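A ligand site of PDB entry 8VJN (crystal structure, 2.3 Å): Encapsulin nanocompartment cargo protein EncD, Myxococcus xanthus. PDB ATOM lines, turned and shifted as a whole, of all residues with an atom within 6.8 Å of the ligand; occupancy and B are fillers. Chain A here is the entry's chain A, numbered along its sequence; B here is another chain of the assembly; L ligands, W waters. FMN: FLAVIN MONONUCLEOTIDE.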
ATOM      1  N   ARG A  19      28.713  -9.768  15.500  1.00  0.00           N
ATOM      2  CA  ARG A  19      27.781 -10.805  15.029  1.00  0.00           C
ATOM      3  C   ARG A  19      27.777 -10.874  13.513  1.00  0.00           C
ATOM      4  O   ARG A  19      27.711 -11.971  12.909  1.00  0.00           O
ATOM      5  CB  ARG A  19      26.354 -10.541  15.562  1.00  0.00           C
ATOM      6  CG  ARG A  19      25.231 -11.366  14.870  1.00  0.00           C
ATOM      7  CD  ARG A  19      23.791 -10.821  15.143  1.00  0.00           C
ATOM      8  NE  ARG A  19      23.654  -9.439  14.669  1.00  0.00           N
ATOM      9  CZ  ARG A  19      23.442  -9.079  13.410  1.00  0.00           C
ATOM     10  NH1 ARG A  19      23.178  -9.976  12.470  1.00  0.00           N
ATOM     11  NH2 ARG A  19      23.506  -7.788  13.082  1.00  0.00           N
ATOM     12  N   ASP A  20      27.876  -9.701  12.879  1.00  0.00           N
ATOM     13  CA  ASP A  20      27.935  -9.616  11.435  1.00  0.00           C
ATOM     14  C   ASP A  20      29.070 -10.451  10.888  1.00  0.00           C
ATOM     15  O   ASP A  20      28.842 -11.303  10.035  1.00  0.00           O
ATOM     16  CB  ASP A  20      28.113  -8.163  11.022  1.00  0.00           C
ATOM     17  CG  ASP A  20      26.818  -7.427  11.039  1.00  0.00           C
ATOM     18  OD1 ASP A  20      25.856  -7.959  10.448  1.00  0.00           O
ATOM     19  OD2 ASP A  20      26.769  -6.313  11.602  1.00  0.00           O
ATOM     20  N   PHE A  21      30.279 -10.253  11.390  1.00  0.00           N
ATOM     21  CA  PHE A  21      31.429 -10.962  10.817  1.00  0.00           C
ATOM     22  C   PHE A  21      31.350 -12.456  11.099  1.00  0.00           C
ATOM     23  O   PHE A  21      31.769 -13.273  10.243  1.00  0.00           O
ATOM     24  CB  PHE A  21      32.737 -10.389  11.339  1.00  0.00           C
ATOM     25  CG  PHE A  21      33.166  -9.155  10.611  1.00  0.00           C
ATOM     26  CD1 PHE A  21      33.677  -9.252   9.338  1.00  0.00           C
ATOM     27  CD2 PHE A  21      33.027  -7.914  11.192  1.00  0.00           C
ATOM     28  CE1 PHE A  21      34.063  -8.126   8.643  1.00  0.00           C
ATOM     29  CE2 PHE A  21      33.424  -6.769  10.504  1.00  0.00           C
ATOM     30  CZ  PHE A  21      33.944  -6.872   9.233  1.00  0.00           C
ATOM     31  N   GLY A  22      30.749 -12.826  12.247  1.00  0.00           N
ATOM     32  CA  GLY A  22      30.512 -14.231  12.511  1.00  0.00           C
ATOM     33  C   GLY A  22      29.631 -14.895  11.479  1.00  0.00           C
ATOM     34  O   GLY A  22      29.728 -16.116  11.270  1.00  0.00           O
ATOM     35  N   TYR A  23      28.735 -14.120  10.832  1.00  0.00           N
ATOM     36  CA  TYR A  23      27.951 -14.646   9.714  1.00  0.00           C
ATOM     37  C   TYR A  23      28.565 -14.344   8.352  1.00  0.00           C
ATOM     38  O   TYR A  23      28.340 -15.098   7.389  1.00  0.00           O
ATOM     39  CB  TYR A  23      26.526 -14.078   9.758  1.00  0.00           C
ATOM     40  CG  TYR A  23      25.657 -14.659  10.874  1.00  0.00           C
ATOM     41  CD1 TYR A  23      24.981 -15.858  10.694  1.00  0.00           C
ATOM     42  CD2 TYR A  23      25.530 -14.003  12.089  1.00  0.00           C
ATOM     43  CE1 TYR A  23      24.219 -16.401  11.713  1.00  0.00           C
ATOM     44  CE2 TYR A  23      24.760 -14.540  13.107  1.00  0.00           C
ATOM     45  CZ  TYR A  23      24.124 -15.740  12.912  1.00  0.00           C
ATOM     46  OH  TYR A  23      23.353 -16.278  13.930  1.00  0.00           O
ATOM     47  N   LEU A  24      29.357 -13.275   8.261  1.00  0.00           N
ATOM     48  CA  LEU A  24      29.871 -12.804   6.982  1.00  0.00           C
ATOM     49  C   LEU A  24      30.892 -13.776   6.424  1.00  0.00           C
ATOM     50  O   LEU A  24      30.830 -14.137   5.238  1.00  0.00           O
ATOM     51  CB  LEU A  24      30.505 -11.417   7.144  1.00  0.00           C
ATOM     52  CG  LEU A  24      31.241 -10.933   5.889  1.00  0.00           C
ATOM     53  CD1 LEU A  24      30.198 -10.521   4.855  1.00  0.00           C
ATOM     54  CD2 LEU A  24      32.172  -9.786   6.141  1.00  0.00           C
ATOM     55  N   MET A  25      31.853 -14.228   7.256  1.00  0.00           N
ATOM     56  CA  MET A  25      32.875 -15.132   6.735  1.00  0.00           C
ATOM     57  C   MET A  25      32.336 -16.491   6.275  1.00  0.00           C
ATOM     58  O   MET A  25      32.752 -16.949   5.182  1.00  0.00           O
ATOM     59  CB  MET A  25      34.015 -15.295   7.751  1.00  0.00           C
ATOM     60  CG  MET A  25      34.675 -13.992   8.156  1.00  0.00           C
ATOM     61  SD  MET A  25      35.307 -13.006   6.785  1.00  0.00           S
ATOM     62  CE  MET A  25      36.032 -11.635   7.673  1.00  0.00           C
ATOM     63  N   PRO A  26      31.441 -17.201   6.991  1.00  0.00           N
ATOM     64  CA  PRO A  26      30.835 -18.413   6.391  1.00  0.00           C
ATOM     65  C   PRO A  26      30.095 -18.144   5.092  1.00  0.00           C
ATOM     66  O   PRO A  26      30.084 -18.997   4.192  1.00  0.00           O
ATOM     67  CB  PRO A  26      29.875 -18.918   7.486  1.00  0.00           C
ATOM     68  CG  PRO A  26      30.421 -18.412   8.736  1.00  0.00           C
ATOM     69  CD  PRO A  26      31.008 -17.054   8.399  1.00  0.00           C
ATOM     70  N   PHE A  27      29.482 -16.962   4.963  1.00  0.00           N
ATOM     71  CA  PHE A  27      28.816 -16.580   3.729  1.00  0.00           C
ATOM     72  C   PHE A  27      29.811 -16.481   2.572  1.00  0.00           C
ATOM     73  O   PHE A  27      29.564 -17.016   1.484  1.00  0.00           O
ATOM     74  CB  PHE A  27      28.067 -15.255   3.939  1.00  0.00           C
ATOM     75  CG  PHE A  27      27.673 -14.587   2.666  1.00  0.00           C
ATOM     76  CD1 PHE A  27      26.847 -15.220   1.754  1.00  0.00           C
ATOM     77  CD2 PHE A  27      28.169 -13.321   2.353  1.00  0.00           C
ATOM     78  CE1 PHE A  27      26.495 -14.588   0.569  1.00  0.00           C
ATOM     79  CE2 PHE A  27      27.805 -12.698   1.139  1.00  0.00           C
ATOM     80  CZ  PHE A  27      26.973 -13.327   0.269  1.00  0.00           C
ATOM     81  N   LEU A  28      30.924 -15.787   2.788  1.00  0.00           N
ATOM     82  CA  LEU A  28      32.006 -15.745   1.793  1.00  0.00           C
ATOM     83  C   LEU A  28      32.458 -17.153   1.397  1.00  0.00           C
ATOM     84  O   LEU A  28      32.714 -17.420   0.218  1.00  0.00           O
ATOM     85  CB  LEU A  28      33.196 -14.940   2.332  1.00  0.00           C
ATOM     86  CG  LEU A  28      32.799 -13.493   2.481  1.00  0.00           C
ATOM     87  CD1 LEU A  28      33.848 -12.704   3.238  1.00  0.00           C
ATOM     88  CD2 LEU A  28      32.561 -12.922   1.089  1.00  0.00           C
ATOM     89  N   ARG A  30      30.595 -19.930   1.452  1.00  0.00           N
ATOM     90  CA  ARG A  30      29.547 -20.508   0.609  1.00  0.00           C
ATOM     91  C   ARG A  30      29.551 -19.928  -0.805  1.00  0.00           C
ATOM     92  O   ARG A  30      29.316 -20.666  -1.778  1.00  0.00           O
ATOM     93  CB  ARG A  30      28.190 -20.333   1.284  1.00  0.00           C
ATOM     94  CG  ARG A  30      28.078 -21.301   2.448  1.00  0.00           C
ATOM     95  CD  ARG A  30      26.726 -21.316   3.071  1.00  0.00           C
ATOM     96  NE  ARG A  30      26.595 -20.232   4.042  1.00  0.00           N
ATOM     97  CZ  ARG A  30      25.810 -19.189   3.830  1.00  0.00           C
ATOM     98  NH1 ARG A  30      25.072 -19.108   2.737  1.00  0.00           N
ATOM     99  NH2 ARG A  30      25.771 -18.209   4.732  1.00  0.00           N
ATOM    100  N   ALA B  16      19.531 -19.090  -3.799  1.00  0.00           N
ATOM    101  CA  ALA B  16      20.009 -19.670  -2.529  1.00  0.00           C
ATOM    102  C   ALA B  16      20.755 -18.593  -1.745  1.00  0.00           C
ATOM    103  O   ALA B  16      21.132 -18.867  -0.592  1.00  0.00           O
ATOM    104  CB  ALA B  16      20.898 -20.850  -2.834  1.00  0.00           C
ATOM    105  N   ARG B  19      18.602 -14.643   0.956  1.00  0.00           N
ATOM    106  CA  ARG B  19      18.660 -14.338   2.385  1.00  0.00           C
ATOM    107  C   ARG B  19      19.985 -13.666   2.734  1.00  0.00           C
ATOM    108  O   ARG B  19      20.017 -12.640   3.448  1.00  0.00           O
ATOM    109  CB  ARG B  19      18.490 -15.634   3.193  1.00  0.00           C
ATOM    110  CG  ARG B  19      18.964 -15.564   4.627  1.00  0.00           C
ATOM    111  CD  ARG B  19      18.231 -16.561   5.517  1.00  0.00           C
ATOM    112  NE  ARG B  19      18.090 -17.871   4.888  1.00  0.00           N
ATOM    113  CZ  ARG B  19      17.327 -18.865   5.357  1.00  0.00           C
ATOM    114  NH1 ARG B  19      16.740 -18.785   6.534  1.00  0.00           N
ATOM    115  NH2 ARG B  19      17.170 -19.961   4.617  1.00  0.00           N
ATOM    116  N   ASP B  20      21.090 -14.209   2.210  1.00  0.00           N
ATOM    117  CA  ASP B  20      22.382 -13.684   2.598  1.00  0.00           C
ATOM    118  C   ASP B  20      22.589 -12.285   2.051  1.00  0.00           C
ATOM    119  O   ASP B  20      23.059 -11.407   2.764  1.00  0.00           O
ATOM    120  CB  ASP B  20      23.501 -14.627   2.189  1.00  0.00           C
ATOM    121  CG  ASP B  20      23.624 -15.812   3.115  1.00  0.00           C
ATOM    122  OD1 ASP B  20      23.794 -15.608   4.333  1.00  0.00           O
ATOM    123  OD2 ASP B  20      23.572 -16.951   2.604  1.00  0.00           O
ATOM    124  N   PHE B  21      22.173 -12.045   0.802  1.00  0.00           N
ATOM    125  CA  PHE B  21      22.236 -10.677   0.316  1.00  0.00           C
ATOM    126  C   PHE B  21      21.287  -9.753   1.076  1.00  0.00           C
ATOM    127  O   PHE B  21      21.603  -8.569   1.291  1.00  0.00           O
ATOM    128  CB  PHE B  21      22.004 -10.645  -1.186  1.00  0.00           C
ATOM    129  CG  PHE B  21      23.169 -11.160  -1.962  1.00  0.00           C
ATOM    130  CD1 PHE B  21      24.356 -10.447  -1.982  1.00  0.00           C
ATOM    131  CD2 PHE B  21      23.133 -12.412  -2.561  1.00  0.00           C
ATOM    132  CE1 PHE B  21      25.472 -10.947  -2.652  1.00  0.00           C
ATOM    133  CE2 PHE B  21      24.232 -12.918  -3.232  1.00  0.00           C
ATOM    134  CZ  PHE B  21      25.407 -12.197  -3.283  1.00  0.00           C
ATOM    135  N   GLY B  22      20.160 -10.317   1.563  1.00  0.00           N
ATOM    136  CA  GLY B  22      19.270  -9.552   2.405  1.00  0.00           C
ATOM    137  C   GLY B  22      19.965  -9.060   3.664  1.00  0.00           C
ATOM    138  O   GLY B  22      19.702  -7.949   4.132  1.00  0.00           O
ATOM    139  N   TYR B  23      20.885  -9.851   4.201  1.00  0.00           N
ATOM    140  CA  TYR B  23      21.678  -9.281   5.301  1.00  0.00           C
ATOM    141  C   TYR B  23      22.826  -8.416   4.794  1.00  0.00           C
ATOM    142  O   TYR B  23      23.201  -7.441   5.455  1.00  0.00           O
ATOM    143  CB  TYR B  23      22.227 -10.385   6.203  1.00  0.00           C
ATOM    144  CG  TYR B  23      21.222 -11.056   7.099  1.00  0.00           C
ATOM    145  CD1 TYR B  23      20.930 -10.560   8.364  1.00  0.00           C
ATOM    146  CD2 TYR B  23      20.545 -12.194   6.662  1.00  0.00           C
ATOM    147  CE1 TYR B  23      19.985 -11.203   9.181  1.00  0.00           C
ATOM    148  CE2 TYR B  23      19.602 -12.839   7.464  1.00  0.00           C
ATOM    149  CZ  TYR B  23      19.328 -12.338   8.717  1.00  0.00           C
ATOM    150  OH  TYR B  23      18.392 -12.978   9.499  1.00  0.00           O
ATOM    151  N   LEU B  24      23.384  -8.757   3.631  1.00  0.00           N
ATOM    152  CA  LEU B  24      24.668  -8.203   3.232  1.00  0.00           C
ATOM    153  C   LEU B  24      24.561  -6.747   2.906  1.00  0.00           C
ATOM    154  O   LEU B  24      25.406  -5.950   3.323  1.00  0.00           O
ATOM    155  CB  LEU B  24      25.226  -8.961   2.018  1.00  0.00           C
ATOM    156  CG  LEU B  24      26.591  -8.453   1.557  1.00  0.00           C
ATOM    157  CD1 LEU B  24      27.658  -8.865   2.537  1.00  0.00           C
ATOM    158  CD2 LEU B  24      26.897  -8.967   0.174  1.00  0.00           C
ATOM    159  N   MET B  25      23.502  -6.365   2.196  1.00  0.00           N
ATOM    160  CA  MET B  25      23.420  -5.003   1.688  1.00  0.00           C
ATOM    161  C   MET B  25      23.275  -3.960   2.820  1.00  0.00           C
ATOM    162  O   MET B  25      24.076  -3.007   2.849  1.00  0.00           O
ATOM    163  CB  MET B  25      22.314  -4.931   0.629  1.00  0.00           C
ATOM    164  CG  MET B  25      22.562  -5.805  -0.576  1.00  0.00           C
ATOM    165  SD  MET B  25      24.071  -5.300  -1.440  1.00  0.00           S
ATOM    166  CE  MET B  25      24.606  -6.815  -2.215  1.00  0.00           C
ATOM    167  N   PHE B  27      24.348  -4.406   5.729  1.00  0.00           N
ATOM    168  CA  PHE B  27      25.649  -4.499   6.381  1.00  0.00           C
ATOM    169  C   PHE B  27      26.692  -3.615   5.684  1.00  0.00           C
ATOM    170  O   PHE B  27      27.424  -2.886   6.357  1.00  0.00           O
ATOM    171  CB  PHE B  27      26.109  -5.953   6.428  1.00  0.00           C
ATOM    172  CG  PHE B  27      27.509  -6.121   6.894  1.00  0.00           C
ATOM    173  CD1 PHE B  27      27.865  -5.795   8.192  1.00  0.00           C
ATOM    174  CD2 PHE B  27      28.484  -6.603   6.022  1.00  0.00           C
ATOM    175  CE1 PHE B  27      29.200  -5.961   8.627  1.00  0.00           C
ATOM    176  CE2 PHE B  27      29.791  -6.760   6.445  1.00  0.00           C
ATOM    177  CZ  PHE B  27      30.147  -6.434   7.743  1.00  0.00           C
ATOM    178  N   ARG B  30      25.951  -0.093   6.660  1.00  0.00           N
ATOM    179  CA  ARG B  30      26.407   0.184   8.020  1.00  0.00           C
ATOM    180  C   ARG B  30      27.928   0.326   8.085  1.00  0.00           C
ATOM    181  O   ARG B  30      28.436   1.187   8.798  1.00  0.00           O
ATOM    182  CB  ARG B  30      25.925  -0.937   8.952  1.00  0.00           C
ATOM    183  CG  ARG B  30      24.452  -0.761   9.372  1.00  0.00           C
ATOM    184  CD  ARG B  30      24.054  -1.751  10.490  1.00  0.00           C
ATOM    185  NE  ARG B  30      23.908  -3.108   9.965  1.00  0.00           N
ATOM    186  CZ  ARG B  30      24.605  -4.159  10.395  1.00  0.00           C
ATOM    187  NH1 ARG B  30      25.475  -4.039  11.387  1.00  0.00           N
ATOM    188  NH2 ARG B  30      24.454  -5.342   9.809  1.00  0.00           N
HETATM  189  N1  FMN L   1      21.303 -14.996   9.861  1.00  0.00           N
HETATM  190  C2  FMN L   1      20.759 -14.979  11.093  1.00  0.00           C
HETATM  191  O2  FMN L   1      19.942 -15.827  11.418  1.00  0.00           O
HETATM  192  N3  FMN L   1      21.091 -14.042  12.011  1.00  0.00           N
HETATM  193  C4  FMN L   1      21.997 -13.058  11.751  1.00  0.00           C
HETATM  194  O4  FMN L   1      22.258 -12.227  12.610  1.00  0.00           O
HETATM  195  C4A FMN L   1      22.590 -13.031  10.485  1.00  0.00           C
HETATM  196  N5  FMN L   1      23.459 -12.090  10.209  1.00  0.00           N
HETATM  197  C5A FMN L   1      24.021 -12.102   8.964  1.00  0.00           C
HETATM  198  C6  FMN L   1      24.960 -11.106   8.650  1.00  0.00           C
HETATM  199  C7  FMN L   1      25.564 -11.053   7.411  1.00  0.00           C
HETATM  200  C7M FMN L   1      26.564  -9.978   7.113  1.00  0.00           C
HETATM  201  C8  FMN L   1      25.238 -12.019   6.433  1.00  0.00           C
HETATM  202  C8M FMN L   1      25.883 -11.976   5.087  1.00  0.00           C
HETATM  203  C9  FMN L   1      24.314 -13.000   6.727  1.00  0.00           C
HETATM  204  C9A FMN L   1      23.687 -13.063   7.984  1.00  0.00           C
HETATM  205  N10 FMN L   1      22.757 -14.040   8.319  1.00  0.00           N
HETATM  206  C10 FMN L   1      22.182 -14.062   9.573  1.00  0.00           C
HETATM  207  C1' FMN L   1      22.372 -15.061   7.331  1.00  0.00           C
HETATM  208  C2' FMN L   1      23.141 -16.347   7.493  1.00  0.00           C
HETATM  209  O2' FMN L   1      24.344 -16.275   6.764  1.00  0.00           O
HETATM  210  C3' FMN L   1      22.300 -17.529   6.992  1.00  0.00           C
HETATM  211  O3' FMN L   1      21.770 -17.212   5.720  1.00  0.00           O
HETATM  212  C4' FMN L   1      21.160 -17.914   7.934  1.00  0.00           C
HETATM  213  O4' FMN L   1      21.705 -18.385   9.174  1.00  0.00           O
HETATM  214  C5' FMN L   1      20.239 -18.967   7.359  1.00  0.00           C
HETATM  215  O5' FMN L   1      20.878 -20.269   7.388  1.00  0.00           O
HETATM  216  P   FMN L   1      20.117 -21.523   6.692  1.00  0.00           P
HETATM  217  O1P FMN L   1      20.244 -21.296   5.201  1.00  0.00           O
HETATM  218  O2P FMN L   1      18.684 -21.466   7.180  1.00  0.00           O
HETATM  219  O3P FMN L   1      20.849 -22.766   7.160  1.00  0.00           O
HETATM  220  O   HOH W   1      19.527 -25.356   5.430  1.00  0.00           O
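OD2 of Asp 20 of chain A lies within salt-bridge range of NH1 of Arg 30 of chain B, 2.6 Å away. The side-chain carboxylate (OD1) of Asp 20 of chain A is in salt-bridge range of the guanidinium group (NH2) of Arg 19 of chain A, 3.5 Å away. NH1 of Arg 30 of chain A is in salt-bridge range of OD2 of Asp 20 of chain B, at 2.6 Å.
Asp 20 of chain A touches the ligand. Tyr 23 of chain A touches the ligand (CB to C5A, 3.3 Å). Phe 27 of chain A touches the ligand (CD2 to C8M, 3.8 Å). CG of Tyr 23 of chain B touches C9A of the ligand, at 3.3 Å. Phe 27 of chain B touches the ligand (CG to C7M, 3.98 Å). Hydrophobic or aromatic side chains that line the ligand: Tyr 23 of chain A, Phe 27 of chain A, Tyr 23 of chain B and Phe 27 of chain B. Of the 21 residues printed, 9 come within 4 Å of the ligand.
NH2 of Arg 19 of chain B is in salt-bridge range of O2P of the ligand (3.3 Å). OD1 of Asp 20 of chain B lies within hydrogen-bond range of O2' of the ligand (2.6 Å). An oxygen (O2') of the ligand is in hydrogen-bond range of the guanidinium group (NH2) of Arg 30 of chain A (3.1 Å). NH1 of Arg 19 of chain A is in hydrogen-bond range of O4 of the ligand (2.4 Å).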
